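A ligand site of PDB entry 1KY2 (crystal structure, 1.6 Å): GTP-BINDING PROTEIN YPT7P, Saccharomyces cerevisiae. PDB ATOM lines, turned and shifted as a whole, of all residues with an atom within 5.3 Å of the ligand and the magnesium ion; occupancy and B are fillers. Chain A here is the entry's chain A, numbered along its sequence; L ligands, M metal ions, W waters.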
ATOM      1  N   GLY A  15      25.359  -9.380  -1.947  1.00  0.00           N
ATOM      2  CA  GLY A  15      24.359  -8.827  -1.031  1.00  0.00           C
ATOM      3  C   GLY A  15      23.935  -9.888   0.016  1.00  0.00           C
ATOM      4  O   GLY A  15      24.204 -11.078  -0.132  1.00  0.00           O
ATOM      5  N   ASP A  16      23.272  -9.393   1.056  1.00  0.00           N
ATOM      6  CA  ASP A  16      22.848 -10.283   2.140  1.00  0.00           C
ATOM      7  C   ASP A  16      21.895 -11.361   1.665  1.00  0.00           C
ATOM      8  O   ASP A  16      21.267 -11.238   0.610  1.00  0.00           O
ATOM      9  CB  ASP A  16      22.162  -9.452   3.232  1.00  0.00           C
ATOM     10  CG  ASP A  16      23.126  -8.618   4.056  1.00  0.00           C
ATOM     11  OD1 ASP A  16      24.357  -8.653   3.864  1.00  0.00           O
ATOM     12  OD2 ASP A  16      22.587  -7.912   4.948  1.00  0.00           O
ATOM     13  N   SER A  17      21.847 -12.458   2.436  1.00  0.00           N
ATOM     14  CA  SER A  17      20.903 -13.514   2.146  1.00  0.00           C
ATOM     15  C   SER A  17      19.476 -12.965   2.167  1.00  0.00           C
ATOM     16  O   SER A  17      19.157 -12.190   3.078  1.00  0.00           O
ATOM     17  CB  SER A  17      21.040 -14.634   3.190  1.00  0.00           C
ATOM     18  OG  SER A  17      20.138 -15.667   2.863  1.00  0.00           O
ATOM     19  N   GLY A  18      18.632 -13.366   1.215  1.00  0.00           N
ATOM     20  CA  GLY A  18      17.226 -12.997   1.307  1.00  0.00           C
ATOM     21  C   GLY A  18      16.916 -11.763   0.478  1.00  0.00           C
ATOM     22  O   GLY A  18      15.718 -11.451   0.387  1.00  0.00           O
ATOM     23  N   VAL A  19      17.901 -11.061  -0.095  1.00  0.00           N
ATOM     24  CA  VAL A  19      17.575  -9.801  -0.757  1.00  0.00           C
ATOM     25  C   VAL A  19      16.995 -10.044  -2.150  1.00  0.00           C
ATOM     26  O   VAL A  19      16.342  -9.112  -2.667  1.00  0.00           O
ATOM     27  CB  VAL A  19      18.788  -8.838  -0.830  1.00  0.00           C
ATOM     28  CG1 VAL A  19      19.261  -8.477   0.583  1.00  0.00           C
ATOM     29  CG2 VAL A  19      19.916  -9.387  -1.683  1.00  0.00           C
ATOM     30  N   GLY A  20      17.187 -11.219  -2.725  1.00  0.00           N
ATOM     31  CA  GLY A  20      16.669 -11.617  -4.014  1.00  0.00           C
ATOM     32  C   GLY A  20      17.683 -11.671  -5.122  1.00  0.00           C
ATOM     33  O   GLY A  20      17.312 -11.492  -6.302  1.00  0.00           O
ATOM     34  N   LYS A  21      18.956 -11.930  -4.846  1.00  0.00           N
ATOM     35  CA  LYS A  21      19.967 -12.039  -5.875  1.00  0.00           C
ATOM     36  C   LYS A  21      19.612 -13.134  -6.882  1.00  0.00           C
ATOM     37  O   LYS A  21      19.644 -12.874  -8.088  1.00  0.00           O
ATOM     38  CB  LYS A  21      21.353 -12.329  -5.278  1.00  0.00           C
ATOM     39  CG  LYS A  21      21.780 -11.322  -4.219  1.00  0.00           C
ATOM     40  CD  LYS A  21      23.175 -11.575  -3.679  1.00  0.00           C
ATOM     41  CE  LYS A  21      23.267 -12.799  -2.767  1.00  0.00           C
ATOM     42  NZ  LYS A  21      22.189 -12.785  -1.717  1.00  0.00           N
ATOM     43  N   THR A  22      19.278 -14.344  -6.411  1.00  0.00           N
ATOM     44  CA  THR A  22      18.944 -15.402  -7.369  1.00  0.00           C
ATOM     45  C   THR A  22      17.700 -15.060  -8.171  1.00  0.00           C
ATOM     46  O   THR A  22      17.647 -15.312  -9.386  1.00  0.00           O
ATOM     47  CB  THR A  22      18.759 -16.729  -6.594  1.00  0.00           C
ATOM     48  OG1 THR A  22      20.013 -17.038  -5.972  1.00  0.00           O
ATOM     49  CG2 THR A  22      18.415 -17.854  -7.552  1.00  0.00           C
ATOM     50  N   SER A  23      16.715 -14.464  -7.510  1.00  0.00           N
ATOM     51  CA  SER A  23      15.508 -14.047  -8.244  1.00  0.00           C
ATOM     52  C   SER A  23      15.828 -13.030  -9.328  1.00  0.00           C
ATOM     53  O   SER A  23      15.284 -13.108 -10.423  1.00  0.00           O
ATOM     54  CB  SER A  23      14.501 -13.449  -7.255  1.00  0.00           C
ATOM     55  OG  SER A  23      14.117 -14.445  -6.321  1.00  0.00           O
ATOM     56  N   LEU A  24      16.731 -12.082  -9.003  1.00  0.00           N
ATOM     57  CA  LEU A  24      17.093 -11.091 -10.012  1.00  0.00           C
ATOM     58  C   LEU A  24      17.825 -11.723 -11.196  1.00  0.00           C
ATOM     59  O   LEU A  24      17.564 -11.383 -12.355  1.00  0.00           O
ATOM     60  CB  LEU A  24      17.981 -10.003  -9.375  1.00  0.00           C
ATOM     61  CG  LEU A  24      17.224  -9.046  -8.451  1.00  0.00           C
ATOM     62  CD1 LEU A  24      18.158  -8.319  -7.487  1.00  0.00           C
ATOM     63  CD2 LEU A  24      16.456  -8.041  -9.311  1.00  0.00           C
ATOM     64  N   TYR A  33      10.253 -16.024 -12.861  1.00  0.00           N
ATOM     65  CA  TYR A  33      10.361 -15.825 -11.423  1.00  0.00           C
ATOM     66  C   TYR A  33       9.724 -17.042 -10.753  1.00  0.00           C
ATOM     67  O   TYR A  33       8.584 -17.397 -11.086  1.00  0.00           O
ATOM     68  CB  TYR A  33       9.645 -14.552 -10.976  1.00  0.00           C
ATOM     69  CG  TYR A  33       9.609 -14.357  -9.474  1.00  0.00           C
ATOM     70  CD1 TYR A  33      10.704 -13.873  -8.789  1.00  0.00           C
ATOM     71  CD2 TYR A  33       8.458 -14.633  -8.749  1.00  0.00           C
ATOM     72  CE1 TYR A  33      10.641 -13.689  -7.425  1.00  0.00           C
ATOM     73  CE2 TYR A  33       8.382 -14.461  -7.388  1.00  0.00           C
ATOM     74  CZ  TYR A  33       9.492 -13.987  -6.725  1.00  0.00           C
ATOM     75  OH  TYR A  33       9.437 -13.805  -5.355  1.00  0.00           O
ATOM     76  N   SER A  34      10.437 -17.643  -9.832  1.00  0.00           N
ATOM     77  CA  SER A  34       9.865 -18.692  -8.993  1.00  0.00           C
ATOM     78  C   SER A  34       9.758 -18.134  -7.574  1.00  0.00           C
ATOM     79  O   SER A  34      10.719 -17.499  -7.137  1.00  0.00           O
ATOM     80  CB  SER A  34      10.730 -19.946  -8.966  1.00  0.00           C
ATOM     81  OG  SER A  34      10.333 -20.794  -7.895  1.00  0.00           O
ATOM     82  N   GLN A  35       8.625 -18.347  -6.913  1.00  0.00           N
ATOM     83  CA  GLN A  35       8.491 -17.833  -5.553  1.00  0.00           C
ATOM     84  C   GLN A  35       9.510 -18.481  -4.621  1.00  0.00           C
ATOM     85  O   GLN A  35       9.926 -17.900  -3.620  1.00  0.00           O
ATOM     86  CB  GLN A  35       7.071 -18.063  -5.030  1.00  0.00           C
ATOM     87  CG  GLN A  35       6.855 -17.243  -3.750  1.00  0.00           C
ATOM     88  CD  GLN A  35       6.431 -15.822  -4.100  1.00  0.00           C
ATOM     89  OE1 GLN A  35       7.129 -14.860  -3.778  1.00  0.00           O
ATOM     90  NE2 GLN A  35       5.283 -15.713  -4.758  1.00  0.00           N
ATOM     91  N   GLN A  36       9.974 -19.700  -4.893  1.00  0.00           N
ATOM     92  CA  GLN A  36      10.899 -20.269  -3.898  1.00  0.00           C
ATOM     93  C   GLN A  36      12.110 -20.929  -4.510  1.00  0.00           C
ATOM     94  O   GLN A  36      12.004 -22.074  -4.973  1.00  0.00           O
ATOM     95  CB  GLN A  36      10.135 -21.287  -3.043  1.00  0.00           C
ATOM     96  CG  GLN A  36       9.040 -20.652  -2.200  1.00  0.00           C
ATOM     97  CD  GLN A  36       8.158 -21.656  -1.471  1.00  0.00           C
ATOM     98  OE1 GLN A  36       8.217 -21.735  -0.249  1.00  0.00           O
ATOM     99  NE2 GLN A  36       7.366 -22.398  -2.221  1.00  0.00           N
ATOM    100  N   TYR A  37      13.237 -20.232  -4.502  1.00  0.00           N
ATOM    101  CA  TYR A  37      14.537 -20.793  -4.852  1.00  0.00           C
ATOM    102  C   TYR A  37      15.236 -21.326  -3.601  1.00  0.00           C
ATOM    103  O   TYR A  37      15.057 -20.796  -2.504  1.00  0.00           O
ATOM    104  CB  TYR A  37      15.470 -19.747  -5.504  1.00  0.00           C
ATOM    105  CG  TYR A  37      14.946 -19.169  -6.799  1.00  0.00           C
ATOM    106  CD1 TYR A  37      14.896 -19.965  -7.944  1.00  0.00           C
ATOM    107  CD2 TYR A  37      14.472 -17.856  -6.859  1.00  0.00           C
ATOM    108  CE1 TYR A  37      14.411 -19.458  -9.136  1.00  0.00           C
ATOM    109  CE2 TYR A  37      13.989 -17.358  -8.054  1.00  0.00           C
ATOM    110  CZ  TYR A  37      13.963 -18.158  -9.182  1.00  0.00           C
ATOM    111  OH  TYR A  37      13.481 -17.669 -10.381  1.00  0.00           O
ATOM    112  N   LYS A  38      16.068 -22.350  -3.740  1.00  0.00           N
ATOM    113  CA  LYS A  38      16.908 -22.738  -2.604  1.00  0.00           C
ATOM    114  C   LYS A  38      17.901 -21.627  -2.301  1.00  0.00           C
ATOM    115  O   LYS A  38      18.309 -20.905  -3.224  1.00  0.00           O
ATOM    116  CB  LYS A  38      17.703 -24.021  -2.869  1.00  0.00           C
ATOM    117  CG  LYS A  38      16.835 -25.260  -3.114  1.00  0.00           C
ATOM    118  CD  LYS A  38      17.736 -26.448  -3.438  1.00  0.00           C
ATOM    119  CE  LYS A  38      18.138 -26.487  -4.899  1.00  0.00           C
ATOM    120  NZ  LYS A  38      17.271 -25.609  -5.751  1.00  0.00           N
ATOM    121  N   ALA A  39      18.274 -21.547  -1.034  1.00  0.00           N
ATOM    122  CA  ALA A  39      19.356 -20.642  -0.674  1.00  0.00           C
ATOM    123  C   ALA A  39      20.588 -20.994  -1.492  1.00  0.00           C
ATOM    124  O   ALA A  39      20.893 -22.170  -1.687  1.00  0.00           O
ATOM    125  CB  ALA A  39      19.687 -20.742   0.822  1.00  0.00           C
ATOM    126  N   THR A  40      21.338 -19.969  -1.926  1.00  0.00           N
ATOM    127  CA  THR A  40      22.489 -20.215  -2.764  1.00  0.00           C
ATOM    128  C   THR A  40      23.701 -20.692  -1.963  1.00  0.00           C
ATOM    129  O   THR A  40      24.017 -20.162  -0.902  1.00  0.00           O
ATOM    130  CB  THR A  40      22.828 -18.945  -3.559  1.00  0.00           C
ATOM    131  OG1 THR A  40      21.649 -18.679  -4.365  1.00  0.00           O
ATOM    132  CG2 THR A  40      23.996 -19.145  -4.498  1.00  0.00           C
ATOM    133  N   ASP A  64      26.050 -15.616  -9.394  1.00  0.00           N
ATOM    134  CA  ASP A  64      25.186 -15.561  -8.236  1.00  0.00           C
ATOM    135  C   ASP A  64      25.906 -16.110  -7.018  1.00  0.00           C
ATOM    136  O   ASP A  64      26.660 -17.083  -7.177  1.00  0.00           O
ATOM    137  CB  ASP A  64      23.935 -16.361  -8.562  1.00  0.00           C
ATOM    138  CG  ASP A  64      22.812 -16.240  -7.547  1.00  0.00           C
ATOM    139  OD1 ASP A  64      22.794 -15.256  -6.771  1.00  0.00           O
ATOM    140  OD2 ASP A  64      21.966 -17.166  -7.565  1.00  0.00           O
ATOM    141  N   THR A  65      25.736 -15.519  -5.853  1.00  0.00           N
ATOM    142  CA  THR A  65      26.569 -15.862  -4.698  1.00  0.00           C
ATOM    143  C   THR A  65      25.758 -16.150  -3.461  1.00  0.00           C
ATOM    144  O   THR A  65      24.581 -15.841  -3.356  1.00  0.00           O
ATOM    145  CB  THR A  65      27.510 -14.685  -4.359  1.00  0.00           C
ATOM    146  OG1 THR A  65      26.754 -13.512  -4.053  1.00  0.00           O
ATOM    147  CG2 THR A  65      28.375 -14.364  -5.577  1.00  0.00           C
ATOM    148  N   ALA A  66      26.420 -16.754  -2.471  1.00  0.00           N
ATOM    149  CA  ALA A  66      25.757 -17.100  -1.230  1.00  0.00           C
ATOM    150  C   ALA A  66      25.798 -15.929  -0.252  1.00  0.00           C
ATOM    151  O   ALA A  66      26.879 -15.491   0.148  1.00  0.00           O
ATOM    152  CB  ALA A  66      26.439 -18.313  -0.607  1.00  0.00           C
ATOM    153  N   GLY A  67      24.604 -15.460   0.119  1.00  0.00           N
ATOM    154  CA  GLY A  67      24.502 -14.382   1.087  1.00  0.00           C
ATOM    155  C   GLY A  67      24.744 -14.896   2.497  1.00  0.00           C
ATOM    156  O   GLY A  67      25.154 -14.131   3.372  1.00  0.00           O
ATOM    157  N   GLN A  68      24.483 -16.167   2.800  1.00  0.00           N
ATOM    158  CA  GLN A  68      24.716 -16.657   4.175  1.00  0.00           C
ATOM    159  C   GLN A  68      26.115 -17.185   4.406  1.00  0.00           C
ATOM    160  O   GLN A  68      26.582 -18.023   3.621  1.00  0.00           O
ATOM    161  CB  GLN A  68      23.756 -17.814   4.511  1.00  0.00           C
ATOM    162  CG  GLN A  68      22.302 -17.494   4.208  1.00  0.00           C
ATOM    163  CD  GLN A  68      21.373 -18.533   4.769  1.00  0.00           C
ATOM    164  OE1 GLN A  68      21.821 -19.286   5.648  1.00  0.00           O
ATOM    165  NE2 GLN A  68      20.146 -18.588   4.293  1.00  0.00           N
ATOM    166  N   ASN A 126      15.960  -3.981  -4.121  1.00  0.00           N
ATOM    167  CA  ASN A 126      14.971  -4.926  -4.637  1.00  0.00           C
ATOM    168  C   ASN A 126      13.742  -5.000  -3.741  1.00  0.00           C
ATOM    169  O   ASN A 126      13.779  -4.551  -2.584  1.00  0.00           O
ATOM    170  CB  ASN A 126      15.640  -6.284  -4.793  1.00  0.00           C
ATOM    171  CG  ASN A 126      14.830  -7.336  -5.515  1.00  0.00           C
ATOM    172  OD1 ASN A 126      14.722  -8.503  -5.092  1.00  0.00           O
ATOM    173  ND2 ASN A 126      14.243  -6.938  -6.639  1.00  0.00           N
ATOM    174  N   LYS A 127      12.666  -5.572  -4.264  1.00  0.00           N
ATOM    175  CA  LYS A 127      11.371  -5.741  -3.609  1.00  0.00           C
ATOM    176  C   LYS A 127      10.584  -4.442  -3.509  1.00  0.00           C
ATOM    177  O   LYS A 127       9.802  -4.218  -2.569  1.00  0.00           O
ATOM    178  CB  LYS A 127      11.520  -6.391  -2.220  1.00  0.00           C
ATOM    179  CG  LYS A 127      12.346  -7.661  -2.246  1.00  0.00           C
ATOM    180  CD  LYS A 127      12.209  -8.521  -1.003  1.00  0.00           C
ATOM    181  CE  LYS A 127      13.292  -9.577  -0.876  1.00  0.00           C
ATOM    182  NZ  LYS A 127      13.194 -10.304   0.428  1.00  0.00           N
ATOM    183  N   ASP A 129       8.105  -3.725  -5.034  1.00  0.00           N
ATOM    184  CA  ASP A 129       6.703  -4.099  -5.072  1.00  0.00           C
ATOM    185  C   ASP A 129       6.108  -4.298  -3.686  1.00  0.00           C
ATOM    186  O   ASP A 129       4.901  -4.504  -3.563  1.00  0.00           O
ATOM    187  CB  ASP A 129       6.535  -5.409  -5.867  1.00  0.00           C
ATOM    188  CG  ASP A 129       7.249  -6.535  -5.130  1.00  0.00           C
ATOM    189  OD1 ASP A 129       8.465  -6.694  -5.344  1.00  0.00           O
ATOM    190  OD2 ASP A 129       6.627  -7.256  -4.306  1.00  0.00           O
ATOM    191  N   ALA A 130       6.888  -4.298  -2.610  1.00  0.00           N
ATOM    192  CA  ALA A 130       6.327  -4.645  -1.303  1.00  0.00           C
ATOM    193  C   ALA A 130       5.309  -3.606  -0.847  1.00  0.00           C
ATOM    194  O   ALA A 130       5.281  -2.489  -1.350  1.00  0.00           O
ATOM    195  CB  ALA A 130       7.425  -4.764  -0.247  1.00  0.00           C
ATOM    196  N   THR A 157      14.040  -2.020  -7.886  1.00  0.00           N
ATOM    197  CA  THR A 157      13.607  -3.135  -8.717  1.00  0.00           C
ATOM    198  C   THR A 157      12.663  -4.094  -8.013  1.00  0.00           C
ATOM    199  O   THR A 157      12.581  -4.145  -6.777  1.00  0.00           O
ATOM    200  CB  THR A 157      14.840  -3.992  -9.140  1.00  0.00           C
ATOM    201  OG1 THR A 157      15.473  -4.533  -7.973  1.00  0.00           O
ATOM    202  CG2 THR A 157      15.847  -3.127  -9.885  1.00  0.00           C
ATOM    203  N   SER A 158      11.999  -4.883  -8.866  1.00  0.00           N
ATOM    204  CA  SER A 158      11.252  -6.041  -8.377  1.00  0.00           C
ATOM    205  C   SER A 158      11.502  -7.226  -9.298  1.00  0.00           C
ATOM    206  O   SER A 158      11.019  -7.266 -10.436  1.00  0.00           O
ATOM    207  CB  SER A 158       9.737  -5.752  -8.288  1.00  0.00           C
ATOM    208  OG  SER A 158       9.047  -6.971  -8.049  1.00  0.00           O
ATOM    209  N   ALA A 159      12.277  -8.223  -8.845  1.00  0.00           N
ATOM    210  CA  ALA A 159      12.390  -9.427  -9.664  1.00  0.00           C
ATOM    211  C   ALA A 159      11.012 -10.096  -9.800  1.00  0.00           C
ATOM    212  O   ALA A 159      10.691 -10.690 -10.816  1.00  0.00           O
ATOM    213  CB  ALA A 159      13.344 -10.417  -9.010  1.00  0.00           C
ATOM    214  N   LYS A 160      10.215 -10.026  -8.734  1.00  0.00           N
ATOM    215  CA  LYS A 160       8.914 -10.701  -8.701  1.00  0.00           C
ATOM    216  C   LYS A 160       7.950 -10.180  -9.754  1.00  0.00           C
ATOM    217  O   LYS A 160       7.320 -10.986 -10.450  1.00  0.00           O
ATOM    218  CB  LYS A 160       8.330 -10.464  -7.306  1.00  0.00           C
ATOM    219  CG  LYS A 160       6.999 -11.155  -7.113  1.00  0.00           C
ATOM    220  CD  LYS A 160       6.582 -11.178  -5.643  1.00  0.00           C
ATOM    221  CE  LYS A 160       5.187 -11.818  -5.541  1.00  0.00           C
ATOM    222  NZ  LYS A 160       5.071 -12.641  -4.302  1.00  0.00           N
ATOM    223  N   ASN A 161       7.839  -8.862  -9.854  1.00  0.00           N
ATOM    224  CA  ASN A 161       6.849  -8.215 -10.721  1.00  0.00           C
ATOM    225  C   ASN A 161       7.497  -7.709 -12.012  1.00  0.00           C
ATOM    226  O   ASN A 161       6.845  -6.997 -12.785  1.00  0.00           O
ATOM    227  CB  ASN A 161       6.184  -7.054  -9.989  1.00  0.00           C
ATOM    228  CG  ASN A 161       5.251  -7.454  -8.867  1.00  0.00           C
ATOM    229  OD1 ASN A 161       4.043  -7.193  -8.868  1.00  0.00           O
ATOM    230  ND2 ASN A 161       5.815  -8.095  -7.850  1.00  0.00           N
HETATM  231  P1  LIG L   1      20.678 -16.266  -0.809  1.00  0.00           P
HETATM  232  O1  LIG L   1      20.897 -17.167  -1.921  1.00  0.00           O
HETATM  233  O2  LIG L   1      21.751 -15.230  -0.635  1.00  0.00           O
HETATM  234  O3  LIG L   1      20.509 -17.127   0.477  1.00  0.00           O
HETATM  235  N1  LIG L   1      19.183 -15.428  -0.978  1.00  0.00           N
HETATM  236  P2  LIG L   1      18.938 -14.521  -2.387  1.00  0.00           P
HETATM  237  O4  LIG L   1      19.463 -13.133  -2.252  1.00  0.00           O
HETATM  238  O5  LIG L   1      19.260 -15.303  -3.618  1.00  0.00           O
HETATM  239  O6  LIG L   1      17.344 -14.382  -2.359  1.00  0.00           O
HETATM  240  P3  LIG L   1      16.227 -15.162  -3.234  1.00  0.00           P
HETATM  241  O7  LIG L   1      16.287 -14.769  -4.747  1.00  0.00           O
HETATM  242  O8  LIG L   1      16.344 -16.660  -2.989  1.00  0.00           O
HETATM  243  O9  LIG L   1      14.841 -14.483  -2.598  1.00  0.00           O
HETATM  244  C1  LIG L   1      14.713 -14.376  -1.230  1.00  0.00           C
HETATM  245  C2  LIG L   1      13.203 -14.084  -0.886  1.00  0.00           C
HETATM  246  O10 LIG L   1      12.999 -12.833  -1.304  1.00  0.00           O
HETATM  247  C3  LIG L   1      12.459 -15.052  -1.317  1.00  0.00           C
HETATM  248  O11 LIG L   1      11.382 -15.140  -0.308  1.00  0.00           O
HETATM  249  C4  LIG L   1      11.991 -14.369  -2.581  1.00  0.00           C
HETATM  250  O12 LIG L   1      10.650 -14.856  -3.061  1.00  0.00           O
HETATM  251  C5  LIG L   1      11.816 -13.182  -2.028  1.00  0.00           C
HETATM  252  N2  LIG L   1      11.883 -12.082  -3.295  1.00  0.00           N
HETATM  253  C6  LIG L   1      12.836 -12.093  -4.290  1.00  0.00           C
HETATM  254  N3  LIG L   1      12.652 -11.115  -5.143  1.00  0.00           N
HETATM  255  C7  LIG L   1      11.530 -10.441  -4.689  1.00  0.00           C
HETATM  256  C8  LIG L   1      10.857  -9.299  -5.218  1.00  0.00           C
HETATM  257  O13 LIG L   1      11.154  -8.646  -6.225  1.00  0.00           O
HETATM  258  N4  LIG L   1       9.759  -8.923  -4.462  1.00  0.00           N
HETATM  259  C9  LIG L   1       9.349  -9.586  -3.315  1.00  0.00           C
HETATM  260  N5  LIG L   1       8.275  -9.107  -2.692  1.00  0.00           N
HETATM  261  N6  LIG L   1       9.968 -10.648  -2.813  1.00  0.00           N
HETATM  262  C10 LIG L   1      11.039 -11.025  -3.550  1.00  0.00           C
HETATM  263 MG    MG M   1      20.386 -17.016  -3.865  1.00  0.00          MG
HETATM  264  O   HOH W   1      22.107 -15.749  -4.327  1.00  0.00           O
HETATM  265  O   HOH W   2      16.388 -18.506  -0.927  1.00  0.00           O
HETATM  266  O   HOH W   3      23.050 -18.234   0.944  1.00  0.00           O
HETATM  267  O   HOH W   4       7.865  -9.043   0.631  1.00  0.00           O
HETATM  268  O   HOH W   5       9.991 -17.739  -0.963  1.00  0.00           O
HETATM  269  O   HOH W   6      13.523 -17.667  -3.343  1.00  0.00           O
HETATM  270  O   HOH W   7      17.905 -17.594   1.153  1.00  0.00           O
HETATM  271  O   HOH W   8       7.721 -12.574  -1.876  1.00  0.00           O
HETATM  272  O   HOH W   9      13.204 -16.670   1.410  1.00  0.00           O
HETATM  273  O   HOH W  10      10.446 -16.943   2.274  1.00  0.00           O
HETATM  274  O   HOH W  11      12.207 -16.024  -5.208  1.00  0.00           O
HETATM  275  O   HOH W  12      18.631 -18.113  -3.685  1.00  0.00           O
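O7 of the ligand is in hydrogen-bond range of N of Thr 22.
The backbone NH of Thr 40 sits close to an oxygen (O1) of the ligand, 2.8 Å away.
N of Ser 23 is in hydrogen-bond range of O7 of the ligand, 2.8 Å away.
OG of Ser 23 sits at hydrogen-bond distance from O7 of the ligand (2.7 Å).
O4 of the ligand is in hydrogen-bond range of N of Lys 21, 2.9 Å away.
O2 of the ligand is in salt-bridge range of NZ of Lys 21 (2.7 Å).
OD1 of Asp 129 is in hydrogen-bond range of N4 of the ligand (2.7 Å).
O12 of the ligand lies within hydrogen-bond range of OH of Tyr 33, 2.8 Å away.
An oxygen (O3) of the ligand is in hydrogen-bond range of the side-chain hydroxyl (OG) of Ser 17 (2.8 Å).
N of Ala 159 sits at hydrogen-bond distance from O13 of the ligand (2.9 Å).
O2 of the ligand lies within hydrogen-bond range of N of Gly 67, 3.0 Å away.
An oxygen (O4) of the ligand sits at hydrogen-bond distance from the backbone NH of Gly 20 (3.0 Å).
N of Lys 160 is in hydrogen-bond range of O13 of the ligand.
An oxygen (O10) of the ligand is in hydrogen-bond range of the side-chain amino group (NZ) of Lys 127 (3.1 Å).
The backbone carbonyl oxygen of Gln 35 lies within hydrogen-bond range of an oxygen (O12) of the ligand (3.2 Å).
The side-chain hydroxyl (OG) of Ser 158 sits at hydrogen-bond distance from an oxygen (O13) of the ligand, at 3.3 Å.
The side-chain amide oxygen of Asn 126 lies close to a nitrogen (N3) of the ligand (3.3 Å).
N of Val 19 sits at hydrogen-bond distance from O4 of the ligand.
Water W1 lies within hydrogen-bond range of the side-chain carboxylate of Asp 64 (2.6 Å) and the backbone carbonyl oxygen of Thr 65 (2.7 Å).
Water W12 lies within hydrogen-bond range of O8 of the ligand (2.8 Å) and O of Lys 38 (2.8 Å).
Water W7 lies within hydrogen-bond range of O3 of the ligand (2.7 Å) and OG of Ser 17 (3.4 Å).
Water W2 bridges an oxygen (O8) of the ligand (2.8 Å) and the backbone carbonyl oxygen of Tyr 37 (3.1 Å).
Water W6 bridges N of Tyr 37 (2.8 Å) and O8 of the ligand (3.0 Å).
Water W5 bridges the backbone carbonyl oxygen (O) of Gln 35 and an oxygen (O11) of the ligand.
The magnesium ion is bound by O1 of the ligand, at 2.0 Å.
O5 of the ligand binds the magnesium ion.
The magnesium ion is bound by water W12.
The magnesium ion is bound by OG1 of Thr 22, at 2.1 Å.
The magnesium ion is bound by OG1 of Thr 40, 2.1 Å away.
The magnesium ion is bound by water W1.
The side-chain carboxylate of Asp 64 sits close to the side-chain hydroxyl of Thr 22.
The side-chain amino group of Lys 21 sits at hydrogen-bond distance from the backbone carbonyl oxygen of Asp 16.
The side-chain amino group of Lys 21 lies within hydrogen-bond range of the backbone carbonyl oxygen of Gly 15, 3.1 Å away.
The side-chain carboxylate (OD1) of Asp 129 lies within hydrogen-bond range of the side-chain hydroxyl (OG) of Ser 158, 2.8 Å away.
The side-chain hydroxyl (OH) of Tyr 33 lies within hydrogen-bond range of the side-chain amide oxygen (OE1) of Gln 35, at 3.0 Å.
The side-chain amide nitrogen of Gln 68 lies close to the side-chain hydroxyl of Ser 17 (3.3 Å).
The backbone carbonyl oxygen (O) of Thr 157 is in hydrogen-bond range of the backbone NH (N) of Lys 127.
The side-chain amide nitrogen of Asn 126 is in hydrogen-bond range of the side-chain hydroxyl of Thr 157, at 3.0 Å.
The backbone NH (N) of Gly 18 sits close to a nitrogen (N1) of the ligand (3.1 Å).
Residues that only touch the ligand: Asp 16, Ala 39 and Thr 65.
Of the 32 residues printed, 20 come within 4 Å of the ligand.
Two residues have an atom within 4 Å of the magnesium ion: Thr 22 and Thr 40.
The nearest printed residue that does not touch the magnesium ion is Asp 64 (4.03 Å).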
